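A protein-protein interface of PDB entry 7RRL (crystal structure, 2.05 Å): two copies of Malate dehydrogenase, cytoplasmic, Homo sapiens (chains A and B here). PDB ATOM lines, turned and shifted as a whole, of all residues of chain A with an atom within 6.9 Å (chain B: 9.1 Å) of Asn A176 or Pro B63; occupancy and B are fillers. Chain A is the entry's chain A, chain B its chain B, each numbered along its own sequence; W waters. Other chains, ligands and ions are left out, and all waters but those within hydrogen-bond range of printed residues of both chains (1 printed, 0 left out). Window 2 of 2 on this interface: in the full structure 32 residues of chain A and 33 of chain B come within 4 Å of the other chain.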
ATOM      1  N   LYS A 164     -11.383 -31.499  18.577  1.00  0.00           N
ATOM      2  CA  LYS A 164     -11.701 -30.241  17.906  1.00  0.00           C
ATOM      3  C   LYS A 164     -12.950 -29.605  18.491  1.00  0.00           C
ATOM      4  O   LYS A 164     -12.976 -28.403  18.787  1.00  0.00           O
ATOM      5  CB  LYS A 164     -11.909 -30.485  16.409  1.00  0.00           C
ATOM      6  CG  LYS A 164     -10.822 -29.963  15.527  1.00  0.00           C
ATOM      7  CD  LYS A 164     -11.032 -30.394  14.084  1.00  0.00           C
ATOM      8  CE  LYS A 164     -11.702 -29.321  13.272  1.00  0.00           C
ATOM      9  NZ  LYS A 164     -11.501 -29.587  11.819  1.00  0.00           N
ATOM     10  N   ALA A 168     -13.485 -25.998  20.186  1.00  0.00           N
ATOM     11  CA  ALA A 168     -14.406 -25.038  19.590  1.00  0.00           C
ATOM     12  C   ALA A 168     -15.483 -24.619  20.581  1.00  0.00           C
ATOM     13  O   ALA A 168     -15.894 -23.451  20.609  1.00  0.00           O
ATOM     14  CB  ALA A 168     -15.033 -25.619  18.327  1.00  0.00           C
ATOM     15  N   VAL A 173     -16.158 -20.879  19.006  1.00  0.00           N
ATOM     16  CA  VAL A 173     -16.001 -20.710  17.568  1.00  0.00           C
ATOM     17  C   VAL A 173     -16.591 -21.926  16.868  1.00  0.00           C
ATOM     18  O   VAL A 173     -17.017 -22.887  17.506  1.00  0.00           O
ATOM     19  CB  VAL A 173     -14.532 -20.499  17.160  1.00  0.00           C
ATOM     20  CG1 VAL A 173     -14.030 -19.149  17.665  1.00  0.00           C
ATOM     21  CG2 VAL A 173     -13.643 -21.648  17.664  1.00  0.00           C
ATOM     22  N   THR A 174     -16.619 -21.872  15.538  1.00  0.00           N
ATOM     23  CA  THR A 174     -17.057 -23.027  14.771  1.00  0.00           C
ATOM     24  C   THR A 174     -15.910 -24.021  14.611  1.00  0.00           C
ATOM     25  O   THR A 174     -14.735 -23.710  14.843  1.00  0.00           O
ATOM     26  CB  THR A 174     -17.581 -22.621  13.391  1.00  0.00           C
ATOM     27  OG1 THR A 174     -16.724 -21.621  12.825  1.00  0.00           O
ATOM     28  CG2 THR A 174     -19.000 -22.084  13.484  1.00  0.00           C
ATOM     29  N   ALA A 175     -16.268 -25.236  14.193  1.00  0.00           N
ATOM     30  CA  ALA A 175     -15.276 -26.301  14.065  1.00  0.00           C
ATOM     31  C   ALA A 175     -14.174 -25.930  13.078  1.00  0.00           C
ATOM     32  O   ALA A 175     -13.003 -26.273  13.282  1.00  0.00           O
ATOM     33  CB  ALA A 175     -15.956 -27.598  13.631  1.00  0.00           C
ATOM     34  N   ASN A 176     -14.531 -25.249  11.992  1.00  0.00           N
ATOM     35  CA  ASN A 176     -13.539 -24.899  10.990  1.00  0.00           C
ATOM     36  C   ASN A 176     -12.571 -23.828  11.472  1.00  0.00           C
ATOM     37  O   ASN A 176     -11.572 -23.577  10.791  1.00  0.00           O
ATOM     38  CB  ASN A 176     -14.237 -24.434   9.719  1.00  0.00           C
ATOM     39  CG  ASN A 176     -14.757 -23.026   9.833  1.00  0.00           C
ATOM     40  OD1 ASN A 176     -15.820 -22.786  10.416  1.00  0.00           O
ATOM     41  ND2 ASN A 176     -14.009 -22.074   9.278  1.00  0.00           N
ATOM     42  N   ASP A 177     -12.839 -23.194  12.618  1.00  0.00           N
ATOM     43  CA  ASP A 177     -11.930 -22.200  13.173  1.00  0.00           C
ATOM     44  C   ASP A 177     -10.806 -22.816  13.999  1.00  0.00           C
ATOM     45  O   ASP A 177      -9.906 -22.085  14.431  1.00  0.00           O
ATOM     46  CB  ASP A 177     -12.706 -21.193  14.023  1.00  0.00           C
ATOM     47  CG  ASP A 177     -13.508 -20.196  13.177  1.00  0.00           C
ATOM     48  OD1 ASP A 177     -13.004 -19.766  12.113  1.00  0.00           O
ATOM     49  OD2 ASP A 177     -14.650 -19.859  13.569  1.00  0.00           O
ATOM     50  N   VAL A 178     -10.822 -24.134  14.210  1.00  0.00           N
ATOM     51  CA  VAL A 178      -9.779 -24.852  14.934  1.00  0.00           C
ATOM     52  C   VAL A 178      -9.080 -25.802  13.970  1.00  0.00           C
ATOM     53  O   VAL A 178      -9.733 -26.405  13.109  1.00  0.00           O
ATOM     54  CB  VAL A 178     -10.377 -25.629  16.129  1.00  0.00           C
ATOM     55  CG1 VAL A 178      -9.307 -26.399  16.857  1.00  0.00           C
ATOM     56  CG2 VAL A 178     -11.075 -24.682  17.079  1.00  0.00           C
ATOM     57  N   LYS A 179      -7.760 -25.959  14.122  1.00  0.00           N
ATOM     58  CA  LYS A 179      -7.023 -26.898  13.279  1.00  0.00           C
ATOM     59  C   LYS A 179      -5.781 -27.406  13.995  1.00  0.00           C
ATOM     60  O   LYS A 179      -5.310 -26.807  14.966  1.00  0.00           O
ATOM     61  CB  LYS A 179      -6.595 -26.262  11.957  1.00  0.00           C
ATOM     62  CG  LYS A 179      -5.348 -25.419  12.109  1.00  0.00           C
ATOM     63  CD  LYS A 179      -4.904 -24.850  10.788  1.00  0.00           C
ATOM     64  CE  LYS A 179      -3.673 -23.994  10.978  1.00  0.00           C
ATOM     65  NZ  LYS A 179      -2.828 -23.992   9.753  1.00  0.00           N
ATOM     66  N   LYS A 201      -8.657 -19.473  15.046  1.00  0.00           N
ATOM     67  CA  LYS A 201      -8.860 -18.090  14.632  1.00  0.00           C
ATOM     68  C   LYS A 201      -9.838 -17.430  15.602  1.00  0.00           C
ATOM     69  O   LYS A 201     -10.942 -17.942  15.812  1.00  0.00           O
ATOM     70  CB  LYS A 201      -9.378 -18.024  13.193  1.00  0.00           C
ATOM     71  N   LYS A 248     -19.126 -40.389  10.328  1.00  0.00           N
ATOM     72  CA  LYS A 248     -18.619 -39.123   9.803  1.00  0.00           C
ATOM     73  C   LYS A 248     -17.096 -39.066   9.874  1.00  0.00           C
ATOM     74  O   LYS A 248     -16.439 -38.534   8.968  1.00  0.00           O
ATOM     75  CB  LYS A 248     -19.227 -37.953  10.560  1.00  0.00           C
ATOM     76  CG  LYS A 248     -19.043 -36.665   9.806  1.00  0.00           C
ATOM     77  CD  LYS A 248     -17.878 -35.880  10.294  1.00  0.00           C
ATOM     78  CE  LYS A 248     -17.642 -34.650   9.400  1.00  0.00           C
ATOM     79  NZ  LYS A 248     -16.537 -33.821   9.975  1.00  0.00           N
ATOM     80  N   GLU A 265      -2.939 -27.766   6.987  1.00  0.00           N
ATOM     81  CA  GLU A 265      -3.459 -28.619   8.039  1.00  0.00           C
ATOM     82  C   GLU A 265      -2.809 -29.982   7.940  1.00  0.00           C
ATOM     83  O   GLU A 265      -2.395 -30.415   6.856  1.00  0.00           O
ATOM     84  CB  GLU A 265      -4.979 -28.801   7.937  1.00  0.00           C
ATOM     85  CG  GLU A 265      -5.793 -27.528   7.931  1.00  0.00           C
ATOM     86  CD  GLU A 265      -7.255 -27.791   8.225  1.00  0.00           C
ATOM     87  OE1 GLU A 265      -7.545 -28.650   9.085  1.00  0.00           O
ATOM     88  OE2 GLU A 265      -8.118 -27.139   7.596  1.00  0.00           O
ATOM     89  N   MET B   1     -21.297 -15.442   5.261  1.00  0.00           N
ATOM     90  CA  MET B   1     -22.324 -16.481   5.333  1.00  0.00           C
ATOM     91  C   MET B   1     -23.681 -15.835   5.527  1.00  0.00           C
ATOM     92  O   MET B   1     -23.777 -14.809   6.195  1.00  0.00           O
ATOM     93  CB  MET B   1     -22.063 -17.434   6.498  1.00  0.00           C
ATOM     94  CG  MET B   1     -20.753 -18.202   6.440  1.00  0.00           C
ATOM     95  SD  MET B   1     -20.924 -19.883   5.799  1.00  0.00           S
ATOM     96  CE  MET B   1     -20.203 -19.677   4.161  1.00  0.00           C
ATOM     97  N   TYR B  22     -27.337 -35.327  10.180  1.00  0.00           N
ATOM     98  CA  TYR B  22     -26.026 -35.064   9.588  1.00  0.00           C
ATOM     99  C   TYR B  22     -26.153 -34.310   8.271  1.00  0.00           C
ATOM    100  O   TYR B  22     -25.434 -33.331   8.034  1.00  0.00           O
ATOM    101  CB  TYR B  22     -25.268 -36.375   9.370  1.00  0.00           C
ATOM    102  CG  TYR B  22     -23.935 -36.212   8.661  1.00  0.00           C
ATOM    103  CD1 TYR B  22     -23.002 -35.269   9.088  1.00  0.00           C
ATOM    104  CD2 TYR B  22     -23.609 -37.009   7.573  1.00  0.00           C
ATOM    105  CE1 TYR B  22     -21.776 -35.122   8.432  1.00  0.00           C
ATOM    106  CE2 TYR B  22     -22.394 -36.880   6.924  1.00  0.00           C
ATOM    107  CZ  TYR B  22     -21.480 -35.933   7.353  1.00  0.00           C
ATOM    108  OH  TYR B  22     -20.272 -35.816   6.694  1.00  0.00           O
ATOM    109  N   ILE B  24     -28.490 -32.352   7.267  1.00  0.00           N
ATOM    110  CA  ILE B  24     -28.855 -30.954   7.526  1.00  0.00           C
ATOM    111  C   ILE B  24     -27.654 -30.186   8.061  1.00  0.00           C
ATOM    112  O   ILE B  24     -27.392 -29.043   7.655  1.00  0.00           O
ATOM    113  CB  ILE B  24     -30.043 -30.869   8.500  1.00  0.00           C
ATOM    114  CG1 ILE B  24     -31.304 -31.447   7.870  1.00  0.00           C
ATOM    115  CG2 ILE B  24     -30.298 -29.416   8.921  1.00  0.00           C
ATOM    116  CD1 ILE B  24     -32.274 -31.957   8.890  1.00  0.00           C
ATOM    117  N   GLY B  25     -26.896 -30.814   8.964  1.00  0.00           N
ATOM    118  CA  GLY B  25     -25.767 -30.151   9.594  1.00  0.00           C
ATOM    119  C   GLY B  25     -24.582 -29.926   8.676  1.00  0.00           C
ATOM    120  O   GLY B  25     -23.832 -28.966   8.868  1.00  0.00           O
ATOM    121  N   ASN B  26     -24.378 -30.802   7.683  1.00  0.00           N
ATOM    122  CA  ASN B  26     -23.182 -30.715   6.858  1.00  0.00           C
ATOM    123  C   ASN B  26     -23.362 -29.813   5.637  1.00  0.00           C
ATOM    124  O   ASN B  26     -22.414 -29.645   4.870  1.00  0.00           O
ATOM    125  CB  ASN B  26     -22.706 -32.128   6.430  1.00  0.00           C
ATOM    126  CG  ASN B  26     -23.648 -32.812   5.420  1.00  0.00           C
ATOM    127  OD1 ASN B  26     -24.522 -32.182   4.834  1.00  0.00           O
ATOM    128  ND2 ASN B  26     -23.456 -34.112   5.218  1.00  0.00           N
ATOM    129  N   GLY B  27     -24.556 -29.242   5.439  1.00  0.00           N
ATOM    130  CA  GLY B  27     -24.819 -28.286   4.388  1.00  0.00           C
ATOM    131  C   GLY B  27     -25.453 -28.845   3.133  1.00  0.00           C
ATOM    132  O   GLY B  27     -25.622 -28.101   2.171  1.00  0.00           O
ATOM    133  N   GLY B  31     -27.607 -25.719   1.661  1.00  0.00           N
ATOM    134  CA  GLY B  31     -26.523 -25.080   0.944  1.00  0.00           C
ATOM    135  C   GLY B  31     -25.277 -24.955   1.804  1.00  0.00           C
ATOM    136  O   GLY B  31     -25.342 -24.825   3.034  1.00  0.00           O
ATOM    137  N   LYS B  32     -24.119 -24.977   1.141  1.00  0.00           N
ATOM    138  CA  LYS B  32     -22.829 -24.963   1.829  1.00  0.00           C
ATOM    139  C   LYS B  32     -22.483 -23.611   2.440  1.00  0.00           C
ATOM    140  O   LYS B  32     -21.483 -23.519   3.163  1.00  0.00           O
ATOM    141  CB  LYS B  32     -21.713 -25.381   0.874  1.00  0.00           C
ATOM    142  N   ASP B  33     -23.277 -22.574   2.175  1.00  0.00           N
ATOM    143  CA  ASP B  33     -23.058 -21.238   2.715  1.00  0.00           C
ATOM    144  C   ASP B  33     -24.159 -20.832   3.688  1.00  0.00           C
ATOM    145  O   ASP B  33     -24.274 -19.650   4.045  1.00  0.00           O
ATOM    146  CB  ASP B  33     -22.944 -20.224   1.576  1.00  0.00           C
ATOM    147  N   GLN B  34     -24.958 -21.794   4.148  1.00  0.00           N
ATOM    148  CA  GLN B  34     -26.116 -21.515   4.991  1.00  0.00           C
ATOM    149  C   GLN B  34     -25.953 -22.102   6.393  1.00  0.00           C
ATOM    150  O   GLN B  34     -26.222 -23.300   6.606  1.00  0.00           O
ATOM    151  CB  GLN B  34     -27.380 -22.064   4.332  1.00  0.00           C
ATOM    152  CG  GLN B  34     -28.593 -21.865   5.176  1.00  0.00           C
ATOM    153  CD  GLN B  34     -28.725 -20.420   5.553  1.00  0.00           C
ATOM    154  OE1 GLN B  34     -28.960 -19.584   4.688  1.00  0.00           O
ATOM    155  NE2 GLN B  34     -28.526 -20.103   6.827  1.00  0.00           N
ATOM    156  N   PRO B  35     -25.542 -21.308   7.382  1.00  0.00           N
ATOM    157  CA  PRO B  35     -25.491 -21.827   8.753  1.00  0.00           C
ATOM    158  C   PRO B  35     -26.880 -22.202   9.257  1.00  0.00           C
ATOM    159  O   PRO B  35     -27.897 -21.614   8.870  1.00  0.00           O
ATOM    160  CB  PRO B  35     -24.887 -20.671   9.560  1.00  0.00           C
ATOM    161  CG  PRO B  35     -24.140 -19.846   8.547  1.00  0.00           C
ATOM    162  CD  PRO B  35     -24.893 -19.992   7.247  1.00  0.00           C
ATOM    163  N   ILE B  36     -26.897 -23.184  10.158  1.00  0.00           N
ATOM    164  CA  ILE B  36     -28.102 -23.848  10.638  1.00  0.00           C
ATOM    165  C   ILE B  36     -28.133 -23.764  12.156  1.00  0.00           C
ATOM    166  O   ILE B  36     -27.139 -24.085  12.813  1.00  0.00           O
ATOM    167  CB  ILE B  36     -28.123 -25.329  10.209  1.00  0.00           C
ATOM    168  CG1 ILE B  36     -28.080 -25.459   8.681  1.00  0.00           C
ATOM    169  CG2 ILE B  36     -29.296 -26.068  10.853  1.00  0.00           C
ATOM    170  CD1 ILE B  36     -29.192 -24.730   7.971  1.00  0.00           C
ATOM    171  N   LEU B  57     -23.624 -34.931  17.392  1.00  0.00           N
ATOM    172  CA  LEU B  57     -23.623 -33.832  16.430  1.00  0.00           C
ATOM    173  C   LEU B  57     -22.453 -32.896  16.674  1.00  0.00           C
ATOM    174  O   LEU B  57     -21.812 -32.427  15.731  1.00  0.00           O
ATOM    175  CB  LEU B  57     -24.943 -33.067  16.508  1.00  0.00           C
ATOM    176  CG  LEU B  57     -26.060 -33.738  15.724  1.00  0.00           C
ATOM    177  CD1 LEU B  57     -27.362 -33.018  15.978  1.00  0.00           C
ATOM    178  CD2 LEU B  57     -25.719 -33.776  14.246  1.00  0.00           C
ATOM    179  N   GLN B  58     -22.175 -32.593  17.938  1.00  0.00           N
ATOM    180  CA  GLN B  58     -20.960 -31.860  18.263  1.00  0.00           C
ATOM    181  C   GLN B  58     -19.728 -32.609  17.781  1.00  0.00           C
ATOM    182  O   GLN B  58     -18.789 -31.998  17.256  1.00  0.00           O
ATOM    183  CB  GLN B  58     -20.888 -31.634  19.768  1.00  0.00           C
ATOM    184  CG  GLN B  58     -21.988 -30.724  20.268  1.00  0.00           C
ATOM    185  CD  GLN B  58     -21.901 -30.473  21.763  1.00  0.00           C
ATOM    186  OE1 GLN B  58     -21.273 -31.238  22.504  1.00  0.00           O
ATOM    187  NE2 GLN B  58     -22.528 -29.387  22.213  1.00  0.00           N
ATOM    188  N   CYS B  60     -19.282 -34.524  15.277  1.00  0.00           N
ATOM    189  CA  CYS B  60     -19.039 -34.437  13.841  1.00  0.00           C
ATOM    190  C   CYS B  60     -18.258 -33.187  13.437  1.00  0.00           C
ATOM    191  O   CYS B  60     -17.819 -33.103  12.286  1.00  0.00           O
ATOM    192  CB  CYS B  60     -20.371 -34.461  13.079  1.00  0.00           C
ATOM    193  SG  CYS B  60     -21.333 -35.983  13.301  1.00  0.00           S
ATOM    194  N   ALA B  61     -18.108 -32.213  14.337  1.00  0.00           N
ATOM    195  CA  ALA B  61     -17.336 -30.994  14.090  1.00  0.00           C
ATOM    196  C   ALA B  61     -17.778 -30.306  12.796  1.00  0.00           C
ATOM    197  O   ALA B  61     -16.996 -30.121  11.862  1.00  0.00           O
ATOM    198  CB  ALA B  61     -15.832 -31.299  14.067  1.00  0.00           C
ATOM    199  N   LEU B  62     -19.065 -29.903  12.775  1.00  0.00           N
ATOM    200  CA  LEU B  62     -19.705 -29.388  11.571  1.00  0.00           C
ATOM    201  C   LEU B  62     -19.654 -27.870  11.554  1.00  0.00           C
ATOM    202  O   LEU B  62     -20.271 -27.235  12.421  1.00  0.00           O
ATOM    203  CB  LEU B  62     -21.143 -29.851  11.502  1.00  0.00           C
ATOM    204  CG  LEU B  62     -21.330 -31.374  11.460  1.00  0.00           C
ATOM    205  CD1 LEU B  62     -22.811 -31.750  11.557  1.00  0.00           C
ATOM    206  CD2 LEU B  62     -20.741 -31.908  10.193  1.00  0.00           C
ATOM    207  N   PRO B  63     -18.968 -27.248  10.586  1.00  0.00           N
ATOM    208  CA  PRO B  63     -18.836 -25.775  10.615  1.00  0.00           C
ATOM    209  C   PRO B  63     -20.153 -25.031  10.467  1.00  0.00           C
ATOM    210  O   PRO B  63     -20.275 -23.913  10.979  1.00  0.00           O
ATOM    211  CB  PRO B  63     -17.896 -25.480   9.437  1.00  0.00           C
ATOM    212  CG  PRO B  63     -18.031 -26.668   8.525  1.00  0.00           C
ATOM    213  CD  PRO B  63     -18.236 -27.846   9.456  1.00  0.00           C
ATOM    214  N   LEU B  64     -21.141 -25.607   9.789  1.00  0.00           N
ATOM    215  CA  LEU B  64     -22.389 -24.905   9.530  1.00  0.00           C
ATOM    216  C   LEU B  64     -23.396 -25.042  10.657  1.00  0.00           C
ATOM    217  O   LEU B  64     -24.443 -24.389  10.622  1.00  0.00           O
ATOM    218  CB  LEU B  64     -23.008 -25.419   8.233  1.00  0.00           C
ATOM    219  CG  LEU B  64     -22.193 -25.014   7.009  1.00  0.00           C
ATOM    220  CD1 LEU B  64     -22.688 -25.734   5.771  1.00  0.00           C
ATOM    221  CD2 LEU B  64     -22.215 -23.501   6.818  1.00  0.00           C
ATOM    222  N   LEU B  65     -23.132 -25.894  11.638  1.00  0.00           N
ATOM    223  CA  LEU B  65     -24.075 -26.101  12.730  1.00  0.00           C
ATOM    224  C   LEU B  65     -23.779 -25.055  13.792  1.00  0.00           C
ATOM    225  O   LEU B  65     -22.976 -25.272  14.695  1.00  0.00           O
ATOM    226  CB  LEU B  65     -23.948 -27.517  13.262  1.00  0.00           C
ATOM    227  CG  LEU B  65     -25.102 -28.130  14.016  1.00  0.00           C
ATOM    228  CD1 LEU B  65     -26.415 -27.903  13.257  1.00  0.00           C
ATOM    229  CD2 LEU B  65     -24.806 -29.621  14.213  1.00  0.00           C
ATOM    230  N   LYS B  66     -24.416 -23.893  13.671  1.00  0.00           N
ATOM    231  CA  LYS B  66     -24.153 -22.821  14.629  1.00  0.00           C
ATOM    232  C   LYS B  66     -24.547 -23.227  16.045  1.00  0.00           C
ATOM    233  O   LYS B  66     -23.800 -22.970  16.995  1.00  0.00           O
ATOM    234  CB  LYS B  66     -24.871 -21.539  14.218  1.00  0.00           C
ATOM    235  CG  LYS B  66     -24.573 -20.364  15.156  1.00  0.00           C
ATOM    236  CD  LYS B  66     -24.385 -19.048  14.408  1.00  0.00           C
ATOM    237  CE  LYS B  66     -24.479 -17.824  15.351  1.00  0.00           C
ATOM    238  NZ  LYS B  66     -25.881 -17.307  15.538  1.00  0.00           N
ATOM    239  N   ASP B  67     -25.701 -23.877  16.205  1.00  0.00           N
ATOM    240  CA  ASP B  67     -26.152 -24.325  17.518  1.00  0.00           C
ATOM    241  C   ASP B  67     -27.136 -25.476  17.349  1.00  0.00           C
ATOM    242  O   ASP B  67     -27.727 -25.655  16.282  1.00  0.00           O
ATOM    243  CB  ASP B  67     -26.794 -23.182  18.307  1.00  0.00           C
ATOM    244  CG  ASP B  67     -26.898 -23.485  19.789  1.00  0.00           C
ATOM    245  OD1 ASP B  67     -26.065 -24.278  20.298  1.00  0.00           O
ATOM    246  OD2 ASP B  67     -27.806 -22.917  20.445  1.00  0.00           O
HETATM  247  O   HOH W   1     -17.024 -31.195   9.324  1.00  0.00           O
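NZ of Lys A248 is in hydrogen-bond range of O of Cys B60 (2.7 Å).
OG1 of Thr A174 sits at hydrogen-bond distance from OD2 of Asp A177.
The side-chain amide oxygen (OD1) of Asn A176 is in hydrogen-bond range of the side-chain hydroxyl (OG1) of Thr A174, at 2.8 Å.
Among the printed residues, pairs that only touch across the chains: Thr A174 with Pro B63 (3.4 Å), Ala A175 with Ala B61 (3.3 Å), Ala A175 with Leu B62 (3.96 Å), Asn A176 with Pro B63 (3.5 Å) and Lys A248 with Tyr B22 (3.4 Å).
Pro B63 touches just these residues of chain A: Thr A174 (3.4 Å) and Asn A176 (3.5 Å).
Ala A175 touches just these residues of chain B: Ala B61 and Leu B62.
No residue of chain B comes within 4 Å of Asp A177.
Of the printed residues of chain A, Ala B61 touches Ala A175.
Printed residues of chain A within 4 Å of Cys B60: Lys A248.
Of the printed residues of chain B, Lys A248 touches Tyr B22 (3.4 Å) and Cys B60 (2.7 Å).
The nearest residue of chain A that does not touch Pro B63 is Ala A175 (4.3 Å).
Of the 22 printed residues of chain B, 5 touch a printed residue of chain A.
Hydrophobic or aromatic side chains of chain B that line the printed part of chain A: Tyr B22, Ala B61 and Pro B63.
Hydrophobic or aromatic side chains of chain A within 4 Å of the printed part of chain B: Ala A175.
Among the printed residues, no Asp or Glu carboxylate lies within 4 Å of a Lys or Arg side-chain nitrogen of the other chain.
No position is printed for both chains.
Water W1 bridges the side-chain amino group of Lys A248 (2.7 Å) and the backbone carbonyl oxygen of Ala B61 (2.8 Å).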
